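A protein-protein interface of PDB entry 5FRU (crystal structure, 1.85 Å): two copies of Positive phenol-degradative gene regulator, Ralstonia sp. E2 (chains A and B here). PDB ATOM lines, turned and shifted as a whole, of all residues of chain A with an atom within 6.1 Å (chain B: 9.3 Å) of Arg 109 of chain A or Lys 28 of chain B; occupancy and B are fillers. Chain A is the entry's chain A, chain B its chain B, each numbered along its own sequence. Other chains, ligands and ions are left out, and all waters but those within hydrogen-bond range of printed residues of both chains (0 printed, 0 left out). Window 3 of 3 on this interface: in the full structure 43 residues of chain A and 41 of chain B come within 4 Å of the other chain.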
ATOM      1  N   THR A 103      21.348   9.407  -9.253  1.00  0.00           N
ATOM      2  CA  THR A 103      20.430   8.957 -10.304  1.00  0.00           C
ATOM      3  C   THR A 103      20.918   9.348 -11.694  1.00  0.00           C
ATOM      4  O   THR A 103      20.859   8.538 -12.624  1.00  0.00           O
ATOM      5  CB  THR A 103      19.028   9.526 -10.073  1.00  0.00           C
ATOM      6  OG1 THR A 103      18.549   9.074  -8.805  1.00  0.00           O
ATOM      7  CG2 THR A 103      18.065   9.071 -11.162  1.00  0.00           C
ATOM      8  N   VAL A 107      23.363   5.243 -11.227  1.00  0.00           N
ATOM      9  CA  VAL A 107      23.732   4.308 -10.179  1.00  0.00           C
ATOM     10  C   VAL A 107      22.501   3.639  -9.577  1.00  0.00           C
ATOM     11  O   VAL A 107      22.477   2.431  -9.365  1.00  0.00           O
ATOM     12  CB  VAL A 107      24.551   5.022  -9.080  1.00  0.00           C
ATOM     13  CG1 VAL A 107      24.651   4.163  -7.839  1.00  0.00           C
ATOM     14  CG2 VAL A 107      25.947   5.383  -9.636  1.00  0.00           C
ATOM     15  N   VAL A 108      21.462   4.425  -9.355  1.00  0.00           N
ATOM     16  CA  VAL A 108      20.309   3.951  -8.624  1.00  0.00           C
ATOM     17  C   VAL A 108      19.201   4.989  -8.780  1.00  0.00           C
ATOM     18  O   VAL A 108      19.480   6.146  -9.067  1.00  0.00           O
ATOM     19  CB  VAL A 108      20.660   3.729  -7.137  1.00  0.00           C
ATOM     20  CG1 VAL A 108      21.133   5.050  -6.481  1.00  0.00           C
ATOM     21  CG2 VAL A 108      19.511   3.095  -6.385  1.00  0.00           C
ATOM     22  N   ARG A 109      17.949   4.571  -8.628  1.00  0.00           N
ATOM     23  CA  ARG A 109      16.832   5.503  -8.604  1.00  0.00           C
ATOM     24  C   ARG A 109      16.383   5.714  -7.156  1.00  0.00           C
ATOM     25  O   ARG A 109      15.933   4.785  -6.483  1.00  0.00           O
ATOM     26  CB  ARG A 109      15.693   4.980  -9.481  1.00  0.00           C
ATOM     27  CG  ARG A 109      14.369   5.688  -9.300  1.00  0.00           C
ATOM     28  CD  ARG A 109      13.254   4.848  -9.914  1.00  0.00           C
ATOM     29  NE  ARG A 109      11.948   5.483  -9.785  1.00  0.00           N
ATOM     30  CZ  ARG A 109      10.856   5.078 -10.427  1.00  0.00           C
ATOM     31  NH1 ARG A 109      10.912   4.032 -11.245  1.00  0.00           N
ATOM     32  NH2 ARG A 109       9.708   5.717 -10.249  1.00  0.00           N
ATOM     33  N   VAL A 110      16.535   6.939  -6.667  1.00  0.00           N
ATOM     34  CA  VAL A 110      16.373   7.217  -5.242  1.00  0.00           C
ATOM     35  C   VAL A 110      15.052   7.915  -4.941  1.00  0.00           C
ATOM     36  O   VAL A 110      14.694   8.887  -5.606  1.00  0.00           O
ATOM     37  CB  VAL A 110      17.531   8.110  -4.697  1.00  0.00           C
ATOM     38  CG1 VAL A 110      17.441   8.254  -3.166  1.00  0.00           C
ATOM     39  CG2 VAL A 110      18.878   7.545  -5.084  1.00  0.00           C
ATOM     40  N   THR A 111      14.336   7.419  -3.936  1.00  0.00           N
ATOM     41  CA  THR A 111      13.154   8.110  -3.426  1.00  0.00           C
ATOM     42  C   THR A 111      13.297   8.365  -1.932  1.00  0.00           C
ATOM     43  O   THR A 111      13.311   7.424  -1.135  1.00  0.00           O
ATOM     44  CB  THR A 111      11.856   7.313  -3.667  1.00  0.00           C
ATOM     45  OG1 THR A 111      11.679   7.078  -5.070  1.00  0.00           O
ATOM     46  CG2 THR A 111      10.651   8.093  -3.124  1.00  0.00           C
ATOM     47  N   LEU A 129      14.525   5.101  -0.338  1.00  0.00           N
ATOM     48  CA  LEU A 129      14.242   3.945  -1.180  1.00  0.00           C
ATOM     49  C   LEU A 129      15.205   3.885  -2.363  1.00  0.00           C
ATOM     50  O   LEU A 129      15.327   4.863  -3.098  1.00  0.00           O
ATOM     51  CB  LEU A 129      12.801   4.021  -1.702  1.00  0.00           C
ATOM     52  CG  LEU A 129      12.306   2.821  -2.500  1.00  0.00           C
ATOM     53  CD1 LEU A 129      12.147   1.823  -1.464  1.00  0.00           C
ATOM     54  CD2 LEU A 129      10.978   3.053  -3.196  1.00  0.00           C
ATOM     55  N   TRP A 130      15.861   2.743  -2.574  1.00  0.00           N
ATOM     56  CA  TRP A 130      16.690   2.542  -3.769  1.00  0.00           C
ATOM     57  C   TRP A 130      16.061   1.548  -4.729  1.00  0.00           C
ATOM     58  O   TRP A 130      15.851   0.397  -4.361  1.00  0.00           O
ATOM     59  CB  TRP A 130      18.082   2.029  -3.409  1.00  0.00           C
ATOM     60  CG  TRP A 130      19.055   3.091  -3.012  1.00  0.00           C
ATOM     61  CD1 TRP A 130      18.901   4.441  -3.154  1.00  0.00           C
ATOM     62  CD2 TRP A 130      20.327   2.894  -2.376  1.00  0.00           C
ATOM     63  NE1 TRP A 130      20.015   5.097  -2.668  1.00  0.00           N
ATOM     64  CE2 TRP A 130      20.898   4.170  -2.178  1.00  0.00           C
ATOM     65  CE3 TRP A 130      21.044   1.763  -1.970  1.00  0.00           C
ATOM     66  CZ2 TRP A 130      22.157   4.347  -1.593  1.00  0.00           C
ATOM     67  CZ3 TRP A 130      22.287   1.939  -1.370  1.00  0.00           C
ATOM     68  CH2 TRP A 130      22.835   3.227  -1.202  1.00  0.00           C
ATOM     69  N   GLU A 131      15.788   1.981  -5.954  1.00  0.00           N
ATOM     70  CA  GLU A 131      15.293   1.073  -6.981  1.00  0.00           C
ATOM     71  C   GLU A 131      16.308   0.944  -8.109  1.00  0.00           C
ATOM     72  O   GLU A 131      16.985   1.919  -8.458  1.00  0.00           O
ATOM     73  CB  GLU A 131      13.947   1.547  -7.518  1.00  0.00           C
ATOM     74  CG  GLU A 131      12.803   1.213  -6.567  1.00  0.00           C
ATOM     75  CD  GLU A 131      11.463   1.650  -7.094  1.00  0.00           C
ATOM     76  OE1 GLU A 131      11.428   2.242  -8.192  1.00  0.00           O
ATOM     77  OE2 GLU A 131      10.445   1.404  -6.412  1.00  0.00           O
ATOM     78  N   ASP A 132      16.416  -0.266  -8.656  1.00  0.00           N
ATOM     79  CA  ASP A 132      17.333  -0.553  -9.761  1.00  0.00           C
ATOM     80  C   ASP A 132      18.796  -0.312  -9.395  1.00  0.00           C
ATOM     81  O   ASP A 132      19.564   0.145 -10.244  1.00  0.00           O
ATOM     82  CB  ASP A 132      17.002   0.297 -10.996  1.00  0.00           C
ATOM     83  CG  ASP A 132      15.559   0.178 -11.428  1.00  0.00           C
ATOM     84  OD1 ASP A 132      15.001  -0.936 -11.341  1.00  0.00           O
ATOM     85  OD2 ASP A 132      14.986   1.203 -11.867  1.00  0.00           O
ATOM     86  N   SER A 133      19.185  -0.619  -8.159  1.00  0.00           N
ATOM     87  CA  SER A 133      20.571  -0.408  -7.725  1.00  0.00           C
ATOM     88  C   SER A 133      21.518  -1.141  -8.654  1.00  0.00           C
ATOM     89  O   SER A 133      21.386  -2.360  -8.840  1.00  0.00           O
ATOM     90  CB  SER A 133      20.795  -0.894  -6.289  1.00  0.00           C
ATOM     91  OG  SER A 133      20.162  -0.053  -5.337  1.00  0.00           O
ATOM     92  N   PHE B  25      20.035   7.812 -21.624  1.00  0.00           N
ATOM     93  CA  PHE B  25      19.833   8.077 -20.206  1.00  0.00           C
ATOM     94  C   PHE B  25      18.392   7.761 -19.827  1.00  0.00           C
ATOM     95  O   PHE B  25      17.462   8.380 -20.337  1.00  0.00           O
ATOM     96  CB  PHE B  25      20.171   9.527 -19.869  1.00  0.00           C
ATOM     97  CG  PHE B  25      21.643   9.798 -19.743  1.00  0.00           C
ATOM     98  CD1 PHE B  25      22.462   9.803 -20.860  1.00  0.00           C
ATOM     99  CD2 PHE B  25      22.204  10.069 -18.505  1.00  0.00           C
ATOM    100  CE1 PHE B  25      23.818  10.062 -20.745  1.00  0.00           C
ATOM    101  CE2 PHE B  25      23.560  10.331 -18.383  1.00  0.00           C
ATOM    102  CZ  PHE B  25      24.366  10.322 -19.506  1.00  0.00           C
ATOM    103  N   ALA B  26      18.218   6.783 -18.944  1.00  0.00           N
ATOM    104  CA  ALA B  26      16.903   6.371 -18.467  1.00  0.00           C
ATOM    105  C   ALA B  26      16.757   6.803 -17.018  1.00  0.00           C
ATOM    106  O   ALA B  26      16.785   5.985 -16.099  1.00  0.00           O
ATOM    107  CB  ALA B  26      16.724   4.876 -18.600  1.00  0.00           C
ATOM    108  N   MET B  27      16.601   8.101 -16.827  1.00  0.00           N
ATOM    109  CA  MET B  27      16.662   8.681 -15.501  1.00  0.00           C
ATOM    110  C   MET B  27      15.552   8.197 -14.573  1.00  0.00           C
ATOM    111  O   MET B  27      15.791   7.950 -13.392  1.00  0.00           O
ATOM    112  CB  MET B  27      16.652  10.207 -15.625  1.00  0.00           C
ATOM    113  CG  MET B  27      17.807  10.739 -16.484  1.00  0.00           C
ATOM    114  SD  MET B  27      19.436  10.679 -15.679  1.00  0.00           S
ATOM    115  CE  MET B  27      20.015   8.983 -15.928  1.00  0.00           C
ATOM    116  N   LYS B  28      14.344   8.027 -15.098  1.00  0.00           N
ATOM    117  CA  LYS B  28      13.235   7.645 -14.232  1.00  0.00           C
ATOM    118  C   LYS B  28      13.376   6.186 -13.808  1.00  0.00           C
ATOM    119  O   LYS B  28      12.666   5.722 -12.917  1.00  0.00           O
ATOM    120  CB  LYS B  28      11.886   7.919 -14.915  1.00  0.00           C
ATOM    121  CG  LYS B  28      11.629   9.421 -15.108  1.00  0.00           C
ATOM    122  CD  LYS B  28      10.304   9.740 -15.807  1.00  0.00           C
ATOM    123  CE  LYS B  28      10.121  11.259 -15.934  1.00  0.00           C
ATOM    124  NZ  LYS B  28       8.857  11.642 -16.631  1.00  0.00           N
ATOM    125  N   GLU B  29      14.315   5.475 -14.428  1.00  0.00           N
ATOM    126  CA  GLU B  29      14.694   4.156 -13.944  1.00  0.00           C
ATOM    127  C   GLU B  29      16.134   4.160 -13.417  1.00  0.00           C
ATOM    128  O   GLU B  29      16.704   3.101 -13.135  1.00  0.00           O
ATOM    129  CB  GLU B  29      14.511   3.097 -15.044  1.00  0.00           C
ATOM    130  CG  GLU B  29      13.044   2.822 -15.471  1.00  0.00           C
ATOM    131  CD  GLU B  29      12.878   1.809 -16.628  1.00  0.00           C
ATOM    132  OE1 GLU B  29      13.874   1.414 -17.278  1.00  0.00           O
ATOM    133  OE2 GLU B  29      11.721   1.403 -16.894  1.00  0.00           O
ATOM    134  N   GLY B  30      16.705   5.356 -13.280  1.00  0.00           N
ATOM    135  CA  GLY B  30      18.031   5.549 -12.701  1.00  0.00           C
ATOM    136  C   GLY B  30      19.158   4.799 -13.394  1.00  0.00           C
ATOM    137  O   GLY B  30      20.050   4.255 -12.742  1.00  0.00           O
ATOM    138  N   SER B  31      19.134   4.752 -14.715  1.00  0.00           N
ATOM    139  CA  SER B  31      20.146   3.963 -15.410  1.00  0.00           C
ATOM    140  C   SER B  31      20.608   4.626 -16.680  1.00  0.00           C
ATOM    141  O   SER B  31      19.946   5.531 -17.215  1.00  0.00           O
ATOM    142  CB  SER B  31      19.617   2.559 -15.705  1.00  0.00           C
ATOM    143  OG  SER B  31      18.366   2.643 -16.351  1.00  0.00           O
ATOM    144  N   ILE B  32      21.774   4.177 -17.142  1.00  0.00           N
ATOM    145  CA  ILE B  32      22.392   4.675 -18.353  1.00  0.00           C
ATOM    146  C   ILE B  32      22.704   3.458 -19.200  1.00  0.00           C
ATOM    147  O   ILE B  32      23.224   2.462 -18.689  1.00  0.00           O
ATOM    148  CB  ILE B  32      23.694   5.473 -18.073  1.00  0.00           C
ATOM    149  CG1 ILE B  32      23.407   6.704 -17.205  1.00  0.00           C
ATOM    150  CG2 ILE B  32      24.376   5.898 -19.369  1.00  0.00           C
ATOM    151  CD1 ILE B  32      24.692   7.450 -16.755  1.00  0.00           C
ATOM    152  N   TRP B  33      22.401   3.544 -20.490  1.00  0.00           N
ATOM    153  CA  TRP B  33      22.568   2.398 -21.365  1.00  0.00           C
ATOM    154  C   TRP B  33      23.416   2.753 -22.571  1.00  0.00           C
ATOM    155  O   TRP B  33      23.277   3.827 -23.161  1.00  0.00           O
ATOM    156  CB  TRP B  33      21.199   1.861 -21.797  1.00  0.00           C
ATOM    157  CG  TRP B  33      20.394   1.412 -20.628  1.00  0.00           C
ATOM    158  CD1 TRP B  33      19.518   2.163 -19.900  1.00  0.00           C
ATOM    159  CD2 TRP B  33      20.415   0.120 -20.025  1.00  0.00           C
ATOM    160  NE1 TRP B  33      18.984   1.413 -18.886  1.00  0.00           N
ATOM    161  CE2 TRP B  33      19.518   0.153 -18.941  1.00  0.00           C
ATOM    162  CE3 TRP B  33      21.098  -1.072 -20.303  1.00  0.00           C
ATOM    163  CZ2 TRP B  33      19.286  -0.953 -18.131  1.00  0.00           C
ATOM    164  CZ3 TRP B  33      20.866  -2.167 -19.499  1.00  0.00           C
ATOM    165  CH2 TRP B  33      19.969  -2.103 -18.429  1.00  0.00           C
ATOM    166  N   ARG B  38      24.487  -1.900 -19.334  1.00  0.00           N
ATOM    167  CA  ARG B  38      24.260  -0.875 -18.330  1.00  0.00           C
ATOM    168  C   ARG B  38      25.600  -0.220 -17.962  1.00  0.00           C
ATOM    169  O   ARG B  38      26.588  -0.917 -17.741  1.00  0.00           O
ATOM    170  CB  ARG B  38      23.585  -1.449 -17.090  1.00  0.00           C
ATOM    171  CG  ARG B  38      23.011  -0.369 -16.214  1.00  0.00           C
ATOM    172  CD  ARG B  38      22.366  -0.924 -14.943  1.00  0.00           C
ATOM    173  NE  ARG B  38      22.036   0.176 -14.051  1.00  0.00           N
ATOM    174  CZ  ARG B  38      21.305   0.066 -12.950  1.00  0.00           C
ATOM    175  NH1 ARG B  38      20.776  -1.106 -12.601  1.00  0.00           N
ATOM    176  NH2 ARG B  38      21.083   1.146 -12.217  1.00  0.00           N
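The side-chain hydroxyl of Thr 103 of chain A sits at hydrogen-bond distance from the backbone carbonyl oxygen of Val 108 of chain A, at 3.1 Å.
NH1 of Arg 109 of chain A lies within salt-bridge range of OE1 of Glu 131 of chain A (3.6 Å).
O of Gly 30 of chain B sits at hydrogen-bond distance from NH2 of Arg 38 of chain B.
Of chain B, only Lys 28 (3.0 Å) and Gly 30 (3.9 Å) come within 4 Å of Arg 109 of chain A.
Lys 28 of chain B touches just one residue of chain A: Arg 109.
Val 108 of chain A touches just one residue of chain B: Gly 30.
Printed residues of chain A within 4 Å of Gly 30 of chain B: Thr 103 (3.8 Å), Val 107 (3.8 Å), Val 108 (3.7 Å) and Arg 109 (3.9 Å).
Printed residues of chain A within 4 Å of Arg 38 of chain B: Val 107 and Asp 132.
Leu 129 of chain A touches none of the printed residues of chain B.
Ala 26 of chain B touches none of the printed residues of chain A.
The nearest residue of chain B that does not touch Arg 109 of chain A is Glu 29 of chain B (4.04 Å).
The nearest residue of chain A that does not touch Lys 28 of chain B is Asp 132 of chain A (5.2 Å).
O of Lys 28 of chain B is in hydrogen-bond range of NH1 of Arg 109 of chain A, 3.0 Å away.
O of Val 107 of chain A sits at hydrogen-bond distance from NH2 of Arg 38 of chain B.
The side-chain carboxylate (OD2) of Asp 132 of chain A sits close to the backbone carbonyl oxygen (O) of Glu 29 of chain B (2.9 Å).
The guanidinium group of Arg 38 of chain B is in hydrogen-bond range of the backbone carbonyl oxygen of Asp 132 of chain A (2.7 Å).
Among the printed residues, pairs that only touch across the chains: Thr 103 of chain A with Met 27 of chain B, Val 108 of chain A with Gly 30 of chain B, Val 107 of chain A with Gly 30 of chain B, Thr 103 of chain A with Gly 30 of chain B and Arg 109 of chain A with Gly 30 of chain B.
No position is printed for both chains.
Of the 10 printed residues of chain B, 5 touch a printed residue of chain A.
Hydrophobic or aromatic side chains of chain B that line the printed part of chain A: Met 27.
Printed residues of chain A that touch a printed residue of chain B: Thr 103, Val 107, Val 108, Arg 109 and Asp 132.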
